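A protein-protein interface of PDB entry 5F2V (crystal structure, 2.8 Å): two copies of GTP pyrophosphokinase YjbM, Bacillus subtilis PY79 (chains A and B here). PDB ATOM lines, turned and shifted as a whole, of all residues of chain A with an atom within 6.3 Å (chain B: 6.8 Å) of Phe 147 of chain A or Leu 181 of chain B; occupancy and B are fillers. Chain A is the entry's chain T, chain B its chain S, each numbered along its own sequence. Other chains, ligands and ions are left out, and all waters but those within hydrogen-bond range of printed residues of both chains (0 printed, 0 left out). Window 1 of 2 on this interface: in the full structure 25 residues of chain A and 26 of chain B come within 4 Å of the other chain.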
ATOM      1  N   ARG A 141      38.234 -25.124 -12.079  1.00  0.00           N
ATOM      2  CA  ARG A 141      37.211 -24.626 -12.992  1.00  0.00           C
ATOM      3  C   ARG A 141      37.237 -23.107 -13.036  1.00  0.00           C
ATOM      4  O   ARG A 141      37.697 -22.460 -12.092  1.00  0.00           O
ATOM      5  CB  ARG A 141      35.835 -25.078 -12.538  1.00  0.00           C
ATOM      6  CG  ARG A 141      35.687 -26.556 -12.383  1.00  0.00           C
ATOM      7  CD  ARG A 141      34.416 -26.853 -11.647  1.00  0.00           C
ATOM      8  NE  ARG A 141      33.991 -28.222 -11.868  1.00  0.00           N
ATOM      9  CZ  ARG A 141      32.728 -28.628 -11.752  1.00  0.00           C
ATOM     10  NH1 ARG A 141      31.762 -27.768 -11.410  1.00  0.00           N
ATOM     11  NH2 ARG A 141      32.420 -29.899 -11.982  1.00  0.00           N
ATOM     12  N   THR A 142      36.742 -22.522 -14.114  1.00  0.00           N
ATOM     13  CA  THR A 142      36.452 -21.099 -14.079  1.00  0.00           C
ATOM     14  C   THR A 142      35.128 -20.889 -13.338  1.00  0.00           C
ATOM     15  O   THR A 142      34.246 -21.753 -13.367  1.00  0.00           O
ATOM     16  CB  THR A 142      36.359 -20.500 -15.484  1.00  0.00           C
ATOM     17  OG1 THR A 142      35.417 -21.259 -16.259  1.00  0.00           O
ATOM     18  CG2 THR A 142      37.710 -20.533 -16.172  1.00  0.00           C
ATOM     19  N   LEU A 143      34.997 -19.755 -12.665  1.00  0.00           N
ATOM     20  CA  LEU A 143      33.703 -19.330 -12.141  1.00  0.00           C
ATOM     21  C   LEU A 143      32.573 -19.525 -13.145  1.00  0.00           C
ATOM     22  O   LEU A 143      31.504 -20.020 -12.784  1.00  0.00           O
ATOM     23  CB  LEU A 143      33.741 -17.866 -11.741  1.00  0.00           C
ATOM     24  CG  LEU A 143      34.533 -17.459 -10.518  1.00  0.00           C
ATOM     25  CD1 LEU A 143      34.611 -15.940 -10.509  1.00  0.00           C
ATOM     26  CD2 LEU A 143      33.796 -17.966  -9.317  1.00  0.00           C
ATOM     27  N   ALA A 144      32.804 -19.140 -14.401  1.00  0.00           N
ATOM     28  CA  ALA A 144      31.757 -19.258 -15.424  1.00  0.00           C
ATOM     29  C   ALA A 144      31.377 -20.711 -15.720  1.00  0.00           C
ATOM     30  O   ALA A 144      30.190 -21.074 -15.695  1.00  0.00           O
ATOM     31  CB  ALA A 144      32.185 -18.561 -16.704  1.00  0.00           C
ATOM     32  N   MET A 145      32.379 -21.542 -16.000  1.00  0.00           N
ATOM     33  CA  MET A 145      32.121 -22.960 -16.231  1.00  0.00           C
ATOM     34  C   MET A 145      31.424 -23.586 -15.025  1.00  0.00           C
ATOM     35  O   MET A 145      30.489 -24.376 -15.188  1.00  0.00           O
ATOM     36  CB  MET A 145      33.418 -23.708 -16.527  1.00  0.00           C
ATOM     37  CG  MET A 145      33.285 -24.810 -17.580  1.00  0.00           C
ATOM     38  SD  MET A 145      32.705 -26.409 -16.958  1.00  0.00           S
ATOM     39  CE  MET A 145      33.354 -26.381 -15.268  1.00  0.00           C
ATOM     40  N   ASN A 146      31.867 -23.226 -13.816  1.00  0.00           N
ATOM     41  CA  ASN A 146      31.281 -23.804 -12.620  1.00  0.00           C
ATOM     42  C   ASN A 146      29.821 -23.429 -12.485  1.00  0.00           C
ATOM     43  O   ASN A 146      29.008 -24.258 -12.082  1.00  0.00           O
ATOM     44  CB  ASN A 146      32.038 -23.384 -11.363  1.00  0.00           C
ATOM     45  CG  ASN A 146      31.443 -23.987 -10.101  1.00  0.00           C
ATOM     46  OD1 ASN A 146      31.376 -25.210  -9.959  1.00  0.00           O
ATOM     47  ND2 ASN A 146      31.000 -23.130  -9.180  1.00  0.00           N
ATOM     48  N   PHE A 147      29.483 -22.183 -12.814  1.00  0.00           N
ATOM     49  CA  PHE A 147      28.078 -21.792 -12.826  1.00  0.00           C
ATOM     50  C   PHE A 147      27.283 -22.735 -13.705  1.00  0.00           C
ATOM     51  O   PHE A 147      26.294 -23.319 -13.256  1.00  0.00           O
ATOM     52  CB  PHE A 147      27.866 -20.368 -13.316  1.00  0.00           C
ATOM     53  CG  PHE A 147      26.442 -19.896 -13.148  1.00  0.00           C
ATOM     54  CD1 PHE A 147      25.635 -20.439 -12.152  1.00  0.00           C
ATOM     55  CD2 PHE A 147      25.892 -18.938 -13.995  1.00  0.00           C
ATOM     56  CE1 PHE A 147      24.313 -20.019 -11.990  1.00  0.00           C
ATOM     57  CE2 PHE A 147      24.563 -18.512 -13.838  1.00  0.00           C
ATOM     58  CZ  PHE A 147      23.776 -19.053 -12.834  1.00  0.00           C
ATOM     59  N   TRP A 148      27.722 -22.902 -14.953  1.00  0.00           N
ATOM     60  CA  TRP A 148      27.006 -23.779 -15.862  1.00  0.00           C
ATOM     61  C   TRP A 148      26.921 -25.199 -15.346  1.00  0.00           C
ATOM     62  O   TRP A 148      25.868 -25.823 -15.417  1.00  0.00           O
ATOM     63  CB  TRP A 148      27.641 -23.799 -17.245  1.00  0.00           C
ATOM     64  CG  TRP A 148      26.881 -24.726 -18.105  1.00  0.00           C
ATOM     65  CD1 TRP A 148      25.694 -24.476 -18.738  1.00  0.00           C
ATOM     66  CD2 TRP A 148      27.192 -26.096 -18.357  1.00  0.00           C
ATOM     67  NE1 TRP A 148      25.265 -25.604 -19.391  1.00  0.00           N
ATOM     68  CE2 TRP A 148      26.171 -26.611 -19.178  1.00  0.00           C
ATOM     69  CE3 TRP A 148      28.243 -26.935 -17.973  1.00  0.00           C
ATOM     70  CZ2 TRP A 148      26.171 -27.920 -19.621  1.00  0.00           C
ATOM     71  CZ3 TRP A 148      28.245 -28.230 -18.422  1.00  0.00           C
ATOM     72  CH2 TRP A 148      27.218 -28.713 -19.235  1.00  0.00           C
ATOM     73  N   ALA A 149      28.034 -25.712 -14.828  1.00  0.00           N
ATOM     74  CA  ALA A 149      28.096 -27.089 -14.349  1.00  0.00           C
ATOM     75  C   ALA A 149      27.125 -27.346 -13.191  1.00  0.00           C
ATOM     76  O   ALA A 149      26.529 -28.418 -13.087  1.00  0.00           O
ATOM     77  CB  ALA A 149      29.499 -27.425 -13.944  1.00  0.00           C
ATOM     78  N   THR A 150      26.967 -26.350 -12.332  1.00  0.00           N
ATOM     79  CA  THR A 150      26.056 -26.452 -11.203  1.00  0.00           C
ATOM     80  C   THR A 150      24.622 -26.672 -11.686  1.00  0.00           C
ATOM     81  O   THR A 150      23.927 -27.575 -11.200  1.00  0.00           O
ATOM     82  CB  THR A 150      26.126 -25.188 -10.323  1.00  0.00           C
ATOM     83  OG1 THR A 150      27.491 -24.912  -9.997  1.00  0.00           O
ATOM     84  CG2 THR A 150      25.313 -25.345  -9.053  1.00  0.00           C
ATOM     85  N   ILE A 151      24.178 -25.852 -12.642  1.00  0.00           N
ATOM     86  CA  ILE A 151      22.834 -26.006 -13.204  1.00  0.00           C
ATOM     87  C   ILE A 151      22.662 -27.357 -13.864  1.00  0.00           C
ATOM     88  O   ILE A 151      21.641 -28.012 -13.676  1.00  0.00           O
ATOM     89  CB  ILE A 151      22.496 -24.947 -14.246  1.00  0.00           C
ATOM     90  CG1 ILE A 151      22.486 -23.569 -13.615  1.00  0.00           C
ATOM     91  CG2 ILE A 151      21.105 -25.176 -14.736  1.00  0.00           C
ATOM     92  CD1 ILE A 151      21.241 -23.328 -12.796  1.00  0.00           C
ATOM     93  N   GLU A 152      23.657 -27.777 -14.636  1.00  0.00           N
ATOM     94  CA  GLU A 152      23.558 -29.056 -15.311  1.00  0.00           C
ATOM     95  C   GLU A 152      23.386 -30.171 -14.296  1.00  0.00           C
ATOM     96  O   GLU A 152      22.604 -31.099 -14.507  1.00  0.00           O
ATOM     97  CB  GLU A 152      24.787 -29.318 -16.170  1.00  0.00           C
ATOM     98  CG  GLU A 152      24.608 -30.515 -17.088  1.00  0.00           C
ATOM     99  CD  GLU A 152      25.693 -31.567 -16.921  1.00  0.00           C
ATOM    100  OE1 GLU A 152      26.835 -31.330 -17.385  1.00  0.00           O
ATOM    101  OE2 GLU A 152      25.389 -32.637 -16.336  1.00  0.00           O
ATOM    102  N   ARG A 173      22.483 -24.086 -24.876  1.00  0.00           N
ATOM    103  CA  ARG A 173      22.625 -22.661 -25.142  1.00  0.00           C
ATOM    104  C   ARG A 173      23.359 -21.961 -24.019  1.00  0.00           C
ATOM    105  O   ARG A 173      24.297 -21.196 -24.275  1.00  0.00           O
ATOM    106  CB  ARG A 173      21.258 -22.006 -25.353  1.00  0.00           C
ATOM    107  CG  ARG A 173      20.527 -22.501 -26.577  1.00  0.00           C
ATOM    108  CD  ARG A 173      19.102 -21.976 -26.636  1.00  0.00           C
ATOM    109  NE  ARG A 173      19.052 -20.524 -26.765  1.00  0.00           N
ATOM    110  CZ  ARG A 173      19.399 -19.875 -27.868  1.00  0.00           C
ATOM    111  NH1 ARG A 173      19.833 -20.562 -28.916  1.00  0.00           N
ATOM    112  NH2 ARG A 173      19.322 -18.549 -27.924  1.00  0.00           N
ATOM    113  N   ALA A 174      22.921 -22.241 -22.785  1.00  0.00           N
ATOM    114  CA  ALA A 174      23.549 -21.713 -21.561  1.00  0.00           C
ATOM    115  C   ALA A 174      25.049 -22.040 -21.489  1.00  0.00           C
ATOM    116  O   ALA A 174      25.860 -21.203 -21.104  1.00  0.00           O
ATOM    117  CB  ALA A 174      22.826 -22.247 -20.320  1.00  0.00           C
ATOM    118  N   SER A 175      25.410 -23.250 -21.893  1.00  0.00           N
ATOM    119  CA  SER A 175      26.802 -23.620 -21.967  1.00  0.00           C
ATOM    120  C   SER A 175      27.612 -22.708 -22.861  1.00  0.00           C
ATOM    121  O   SER A 175      28.684 -22.264 -22.477  1.00  0.00           O
ATOM    122  CB  SER A 175      26.944 -25.048 -22.460  1.00  0.00           C
ATOM    123  OG  SER A 175      28.311 -25.421 -22.446  1.00  0.00           O
ATOM    124  N   ALA A 177      26.960 -19.759 -23.798  1.00  0.00           N
ATOM    125  CA  ALA A 177      26.968 -18.436 -23.219  1.00  0.00           C
ATOM    126  C   ALA A 177      28.123 -18.337 -22.231  1.00  0.00           C
ATOM    127  O   ALA A 177      28.952 -17.432 -22.315  1.00  0.00           O
ATOM    128  CB  ALA A 177      25.652 -18.153 -22.556  1.00  0.00           C
ATOM    129  N   ALA A 178      28.188 -19.297 -21.313  1.00  0.00           N
ATOM    130  CA  ALA A 178      29.272 -19.366 -20.332  1.00  0.00           C
ATOM    131  C   ALA A 178      30.623 -19.421 -21.010  1.00  0.00           C
ATOM    132  O   ALA A 178      31.525 -18.673 -20.661  1.00  0.00           O
ATOM    133  CB  ALA A 178      29.094 -20.570 -19.422  1.00  0.00           C
ATOM    134  N   LEU A 181      31.302 -15.880 -22.221  1.00  0.00           N
ATOM    135  CA  LEU A 181      31.711 -15.044 -21.093  1.00  0.00           C
ATOM    136  C   LEU A 181      33.195 -15.223 -20.729  1.00  0.00           C
ATOM    137  O   LEU A 181      33.884 -14.251 -20.446  1.00  0.00           O
ATOM    138  CB  LEU A 181      30.844 -15.326 -19.870  1.00  0.00           C
ATOM    139  CG  LEU A 181      31.166 -14.372 -18.718  1.00  0.00           C
ATOM    140  CD1 LEU A 181      31.131 -12.940 -19.225  1.00  0.00           C
ATOM    141  CD2 LEU A 181      30.194 -14.545 -17.569  1.00  0.00           C
ATOM    142  N   GLU B  39      22.141 -17.959  -3.413  1.00  0.00           N
ATOM    143  CA  GLU B  39      23.208 -18.891  -3.685  1.00  0.00           C
ATOM    144  C   GLU B  39      24.300 -18.745  -2.622  1.00  0.00           C
ATOM    145  O   GLU B  39      24.699 -19.731  -2.020  1.00  0.00           O
ATOM    146  CB  GLU B  39      23.754 -18.667  -5.087  1.00  0.00           C
ATOM    147  CG  GLU B  39      24.752 -19.709  -5.535  1.00  0.00           C
ATOM    148  CD  GLU B  39      24.142 -21.102  -5.733  1.00  0.00           C
ATOM    149  OE1 GLU B  39      22.893 -21.228  -5.909  1.00  0.00           O
ATOM    150  OE2 GLU B  39      24.945 -22.071  -5.705  1.00  0.00           O
ATOM    151  N   CYS B  78      22.458 -14.453  -6.301  1.00  0.00           N
ATOM    152  CA  CYS B  78      21.439 -15.394  -6.768  1.00  0.00           C
ATOM    153  C   CYS B  78      21.784 -16.063  -8.099  1.00  0.00           C
ATOM    154  O   CYS B  78      22.462 -15.475  -8.946  1.00  0.00           O
ATOM    155  CB  CYS B  78      20.104 -14.699  -6.929  1.00  0.00           C
ATOM    156  SG  CYS B  78      19.715 -13.622  -5.602  1.00  0.00           S
ATOM    157  N   GLN B  79      21.285 -17.284  -8.278  1.00  0.00           N
ATOM    158  CA  GLN B  79      21.474 -18.040  -9.511  1.00  0.00           C
ATOM    159  C   GLN B  79      20.720 -17.437 -10.698  1.00  0.00           C
ATOM    160  O   GLN B  79      21.249 -17.316 -11.807  1.00  0.00           O
ATOM    161  CB  GLN B  79      21.013 -19.474  -9.302  1.00  0.00           C
ATOM    162  CG  GLN B  79      21.904 -20.527  -9.909  1.00  0.00           C
ATOM    163  CD  GLN B  79      21.818 -21.827  -9.150  1.00  0.00           C
ATOM    164  OE1 GLN B  79      20.734 -22.375  -8.966  1.00  0.00           O
ATOM    165  NE2 GLN B  79      22.959 -22.313  -8.672  1.00  0.00           N
ATOM    166  N   PHE B  80      19.477 -17.051 -10.446  1.00  0.00           N
ATOM    167  CA  PHE B  80      18.600 -16.567 -11.491  1.00  0.00           C
ATOM    168  C   PHE B  80      18.138 -15.141 -11.263  1.00  0.00           C
ATOM    169  O   PHE B  80      17.928 -14.724 -10.134  1.00  0.00           O
ATOM    170  CB  PHE B  80      17.380 -17.467 -11.594  1.00  0.00           C
ATOM    171  CG  PHE B  80      17.698 -18.869 -11.982  1.00  0.00           C
ATOM    172  CD1 PHE B  80      18.172 -19.158 -13.245  1.00  0.00           C
ATOM    173  CD2 PHE B  80      17.499 -19.905 -11.099  1.00  0.00           C
ATOM    174  CE1 PHE B  80      18.452 -20.458 -13.612  1.00  0.00           C
ATOM    175  CE2 PHE B  80      17.782 -21.198 -11.457  1.00  0.00           C
ATOM    176  CZ  PHE B  80      18.260 -21.476 -12.715  1.00  0.00           C
ATOM    177  N   ARG B 115      18.924  -7.570 -12.820  1.00  0.00           N
ATOM    178  CA  ARG B 115      20.116  -8.373 -12.505  1.00  0.00           C
ATOM    179  C   ARG B 115      20.896  -7.862 -11.263  1.00  0.00           C
ATOM    180  O   ARG B 115      21.899  -8.468 -10.825  1.00  0.00           O
ATOM    181  CB  ARG B 115      21.059  -8.426 -13.716  1.00  0.00           C
ATOM    182  CG  ARG B 115      20.576  -9.314 -14.865  1.00  0.00           C
ATOM    183  CD  ARG B 115      21.736  -9.828 -15.734  1.00  0.00           C
ATOM    184  NE  ARG B 115      22.842  -8.873 -15.860  1.00  0.00           N
ATOM    185  CZ  ARG B 115      24.113  -9.228 -16.060  1.00  0.00           C
ATOM    186  NH1 ARG B 115      24.427 -10.508 -16.157  1.00  0.00           N
ATOM    187  NH2 ARG B 115      25.081  -8.315 -16.164  1.00  0.00           N
ATOM    188  N   THR B 142      22.958 -11.376  -9.475  1.00  0.00           N
ATOM    189  CA  THR B 142      23.079 -12.732  -9.998  1.00  0.00           C
ATOM    190  C   THR B 142      24.558 -13.086  -9.992  1.00  0.00           C
ATOM    191  O   THR B 142      25.388 -12.198 -10.003  1.00  0.00           O
ATOM    192  CB  THR B 142      22.539 -12.870 -11.432  1.00  0.00           C
ATOM    193  OG1 THR B 142      23.400 -12.157 -12.329  1.00  0.00           O
ATOM    194  CG2 THR B 142      21.138 -12.325 -11.549  1.00  0.00           C
ATOM    195  N   LEU B 143      24.893 -14.372  -9.985  1.00  0.00           N
ATOM    196  CA  LEU B 143      26.293 -14.798 -10.023  1.00  0.00           C
ATOM    197  C   LEU B 143      27.024 -14.142 -11.179  1.00  0.00           C
ATOM    198  O   LEU B 143      28.037 -13.480 -10.981  1.00  0.00           O
ATOM    199  CB  LEU B 143      26.390 -16.317 -10.131  1.00  0.00           C
ATOM    200  CG  LEU B 143      25.925 -17.116  -8.907  1.00  0.00           C
ATOM    201  CD1 LEU B 143      26.023 -18.601  -9.154  1.00  0.00           C
ATOM    202  CD2 LEU B 143      26.752 -16.752  -7.704  1.00  0.00           C
ATOM    203  N   ALA B 144      26.492 -14.303 -12.386  1.00  0.00           N
ATOM    204  CA  ALA B 144      27.069 -13.700 -13.585  1.00  0.00           C
ATOM    205  C   ALA B 144      27.327 -12.208 -13.410  1.00  0.00           C
ATOM    206  O   ALA B 144      28.460 -11.742 -13.568  1.00  0.00           O
ATOM    207  CB  ALA B 144      26.168 -13.925 -14.746  1.00  0.00           C
ATOM    208  N   GLU B 176      28.155  -7.609 -21.539  1.00  0.00           N
ATOM    209  CA  GLU B 176      27.071  -8.084 -22.395  1.00  0.00           C
ATOM    210  C   GLU B 176      27.087  -9.604 -22.449  1.00  0.00           C
ATOM    211  O   GLU B 176      26.041 -10.238 -22.552  1.00  0.00           O
ATOM    212  CB  GLU B 176      27.174  -7.463 -23.796  1.00  0.00           C
ATOM    213  CG  GLU B 176      26.182  -8.010 -24.856  1.00  0.00           C
ATOM    214  CD  GLU B 176      24.691  -8.120 -24.392  1.00  0.00           C
ATOM    215  OE1 GLU B 176      24.178  -7.193 -23.707  1.00  0.00           O
ATOM    216  OE2 GLU B 176      24.024  -9.140 -24.747  1.00  0.00           O
ATOM    217  N   ALA B 177      28.274 -10.192 -22.336  1.00  0.00           N
ATOM    218  CA  ALA B 177      28.399 -11.651 -22.255  1.00  0.00           C
ATOM    219  C   ALA B 177      27.698 -12.209 -21.018  1.00  0.00           C
ATOM    220  O   ALA B 177      27.077 -13.275 -21.070  1.00  0.00           O
ATOM    221  CB  ALA B 177      29.852 -12.056 -22.246  1.00  0.00           C
ATOM    222  N   ALA B 178      27.810 -11.482 -19.909  1.00  0.00           N
ATOM    223  CA  ALA B 178      27.256 -11.924 -18.644  1.00  0.00           C
ATOM    224  C   ALA B 178      25.751 -11.891 -18.735  1.00  0.00           C
ATOM    225  O   ALA B 178      25.067 -12.823 -18.307  1.00  0.00           O
ATOM    226  CB  ALA B 178      27.758 -11.051 -17.492  1.00  0.00           C
ATOM    227  N   SER B 179      25.237 -10.817 -19.308  1.00  0.00           N
ATOM    228  CA  SER B 179      23.805 -10.684 -19.508  1.00  0.00           C
ATOM    229  C   SER B 179      23.208 -11.804 -20.366  1.00  0.00           C
ATOM    230  O   SER B 179      22.136 -12.298 -20.043  1.00  0.00           O
ATOM    231  CB  SER B 179      23.494  -9.327 -20.123  1.00  0.00           C
ATOM    232  OG  SER B 179      24.048  -8.293 -19.325  1.00  0.00           O
ATOM    233  N   ARG B 180      23.884 -12.228 -21.436  1.00  0.00           N
ATOM    234  CA  ARG B 180      23.350 -13.346 -22.222  1.00  0.00           C
ATOM    235  C   ARG B 180      23.274 -14.589 -21.349  1.00  0.00           C
ATOM    236  O   ARG B 180      22.261 -15.284 -21.350  1.00  0.00           O
ATOM    237  CB  ARG B 180      24.185 -13.632 -23.483  1.00  0.00           C
ATOM    238  CG  ARG B 180      24.215 -12.477 -24.475  1.00  0.00           C
ATOM    239  CD  ARG B 180      25.530 -12.413 -25.271  1.00  0.00           C
ATOM    240  NE  ARG B 180      25.582 -11.250 -26.166  1.00  0.00           N
ATOM    241  CZ  ARG B 180      24.904 -11.149 -27.315  1.00  0.00           C
ATOM    242  NH1 ARG B 180      24.104 -12.144 -27.715  1.00  0.00           N
ATOM    243  NH2 ARG B 180      25.023 -10.052 -28.073  1.00  0.00           N
ATOM    244  N   LEU B 181      24.343 -14.859 -20.604  1.00  0.00           N
ATOM    245  CA  LEU B 181      24.367 -16.001 -19.707  1.00  0.00           C
ATOM    246  C   LEU B 181      23.151 -16.028 -18.790  1.00  0.00           C
ATOM    247  O   LEU B 181      22.503 -17.061 -18.625  1.00  0.00           O
ATOM    248  CB  LEU B 181      25.626 -15.996 -18.871  1.00  0.00           C
ATOM    249  CG  LEU B 181      25.590 -17.215 -17.964  1.00  0.00           C
ATOM    250  CD1 LEU B 181      25.475 -18.443 -18.858  1.00  0.00           C
ATOM    251  CD2 LEU B 181      26.829 -17.259 -17.090  1.00  0.00           C
ATOM    252  N   ASP B 182      22.830 -14.878 -18.217  1.00  0.00           N
ATOM    253  CA  ASP B 182      21.647 -14.768 -17.388  1.00  0.00           C
ATOM    254  C   ASP B 182      20.348 -14.962 -18.143  1.00  0.00           C
ATOM    255  O   ASP B 182      19.424 -15.606 -17.658  1.00  0.00           O
ATOM    256  CB  ASP B 182      21.625 -13.418 -16.701  1.00  0.00           C
ATOM    257  CG  ASP B 182      22.312 -13.454 -15.384  1.00  0.00           C
ATOM    258  OD1 ASP B 182      22.265 -14.528 -14.752  1.00  0.00           O
ATOM    259  OD2 ASP B 182      22.901 -12.436 -14.985  1.00  0.00           O
ATOM    260  N   GLU B 183      20.264 -14.380 -19.330  1.00  0.00           N
ATOM    261  CA  GLU B 183      19.056 -14.505 -20.132  1.00  0.00           C
ATOM    262  C   GLU B 183      18.857 -15.981 -20.498  1.00  0.00           C
ATOM    263  O   GLU B 183      17.787 -16.549 -20.280  1.00  0.00           O
ATOM    264  CB  GLU B 183      19.143 -13.598 -21.361  1.00  0.00           C
ATOM    265  CG  GLU B 183      19.011 -12.108 -21.036  1.00  0.00           C
ATOM    266  CD  GLU B 183      19.731 -11.188 -22.032  1.00  0.00           C
ATOM    267  OE1 GLU B 183      20.250 -11.685 -23.066  1.00  0.00           O
ATOM    268  OE2 GLU B 183      19.781  -9.958 -21.773  1.00  0.00           O
ATOM    269  N   GLU B 184      19.902 -16.620 -21.006  1.00  0.00           N
ATOM    270  CA  GLU B 184      19.844 -18.060 -21.230  1.00  0.00           C
ATOM    271  C   GLU B 184      19.435 -18.779 -19.959  1.00  0.00           C
ATOM    272  O   GLU B 184      18.525 -19.602 -19.994  1.00  0.00           O
ATOM    273  CB  GLU B 184      21.178 -18.594 -21.736  1.00  0.00           C
ATOM    274  CG  GLU B 184      21.509 -18.141 -23.151  1.00  0.00           C
ATOM    275  CD  GLU B 184      20.332 -18.275 -24.107  1.00  0.00           C
ATOM    276  OE1 GLU B 184      19.608 -19.299 -24.061  1.00  0.00           O
ATOM    277  OE2 GLU B 184      20.120 -17.343 -24.904  1.00  0.00           O
ATOM    278  N   MET B 185      20.071 -18.435 -18.834  1.00  0.00           N
ATOM    279  CA  MET B 185      19.708 -19.041 -17.542  1.00  0.00           C
ATOM    280  C   MET B 185      18.211 -18.899 -17.214  1.00  0.00           C
ATOM    281  O   MET B 185      17.586 -19.878 -16.813  1.00  0.00           O
ATOM    282  CB  MET B 185      20.541 -18.456 -16.386  1.00  0.00           C
ATOM    283  CG  MET B 185      21.988 -18.980 -16.220  1.00  0.00           C
ATOM    284  SD  MET B 185      22.307 -20.753 -16.479  1.00  0.00           S
ATOM    285  CE  MET B 185      20.947 -21.528 -15.616  1.00  0.00           C
ATOM    286  N   SER B 186      17.633 -17.709 -17.392  1.00  0.00           N
ATOM    287  CA  SER B 186      16.197 -17.516 -17.129  1.00  0.00           C
ATOM    288  C   SER B 186      15.293 -18.399 -17.999  1.00  0.00           C
ATOM    289  O   SER B 186      14.202 -18.778 -17.569  1.00  0.00           O
ATOM    290  CB  SER B 186      15.777 -16.058 -17.325  1.00  0.00           C
ATOM    291  OG  SER B 186      16.840 -15.169 -17.084  1.00  0.00           O
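NE of Arg 173 of chain A is in salt-bridge range of OE1 of Glu 184 of chain B (3.0 Å).
The side-chain amide nitrogen (NE2) of Gln 79 of chain B lies within hydrogen-bond range of the side-chain carboxylate (OE1) of Glu 39 of chain B. The guanidinium group of Arg 115 of chain B lies close to the backbone carbonyl oxygen of Ala 178 of chain B, 3.2 Å away. O of Cys 78 of chain B lies within hydrogen-bond range of N of Leu 143 of chain B (2.9 Å). O of Asn 146 of chain A sits at hydrogen-bond distance from OG1 of Thr 150 of chain A (2.7 Å).
CE1 of Phe 147 of chain A touches CG of Gln 79 of chain B (3.2 Å). CD1 of Phe 147 of chain A touches CD1 of Leu 143 of chain B (3.5 Å). Gln 79 of chain B touches Thr 150 of chain A (NE2 to CG2, 3.9 Å). OE1 of Gln 79 of chain B touches CD1 of Ile 151 of chain A, 3.98 Å away. CG1 of Ile 151 of chain A touches CE of Met 185 of chain B, 3.2 Å away. Ala 174 of chain A touches Leu 181 of chain B. Ala 174 of chain A touches Glu 184 of chain B. Ala 177 of chain A touches Leu 181 of chain B (CB to CD1, 3.7 Å). Ala 178 of chain A touches Leu 181 of chain B (N to CD1, 3.8 Å). Leu 181 of chain A touches Ala 178 of chain B (CD1 to N, 3.7 Å).
Of chain B, only Gln 79, Leu 143, Leu 181 and Met 185 come within 4 Å of Phe 147 of chain A. Printed residues of chain B within 4 Å of Thr 150 of chain A: Gln 79 (3.9 Å). Glu 152 of chain A touches none of the printed residues of chain B. Of the printed residues of chain A, Phe 80 of chain B touches Ile 151 (3.5 Å). Of the printed residues of chain A, Ala 177 of chain B touches Leu 181 (3.4 Å). Of the printed residues of chain A, Ala 178 of chain B touches Leu 181 (3.7 Å). Ser 179 of chain B touches none of the printed residues of chain A. Of the printed residues of chain A, Leu 181 of chain B touches Phe 147 (3.6 Å), Ala 174 (3.6 Å), Ala 177 (3.7 Å) and Ala 178 (3.8 Å). Of the printed residues of chain A, Met 185 of chain B touches Phe 147 (3.5 Å) and Ile 151 (3.2 Å). The nearest residue of chain B that does not touch Phe 147 of chain A is Asp 182 of chain B (4.7 Å).
Of the 19 printed residues of chain B, 8 touch a printed residue of chain A. Of the 18 printed residues of chain A, 8 touch a printed residue of chain B. Hydrophobic or aromatic side chains of chain A within 4 Å of the printed part of chain B: Phe 147, Ile 151, Ala 177 and Leu 181.
Ala 177 of chain A touches Leu 181 of chain B, and with the chains exchanged Leu 181 of chain A touches Ala 177 of chain B. Ala 178 of chain A touches Leu 181 of chain B, and with the chains exchanged Leu 181 of chain A touches Ala 178 of chain B. Positions printed for both chains: 142, 143, 144, 177, 178 and 181. Of the 15 pairs that touch across the chains among the printed residues, 4 have their exchanged pair printed and touching as well.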
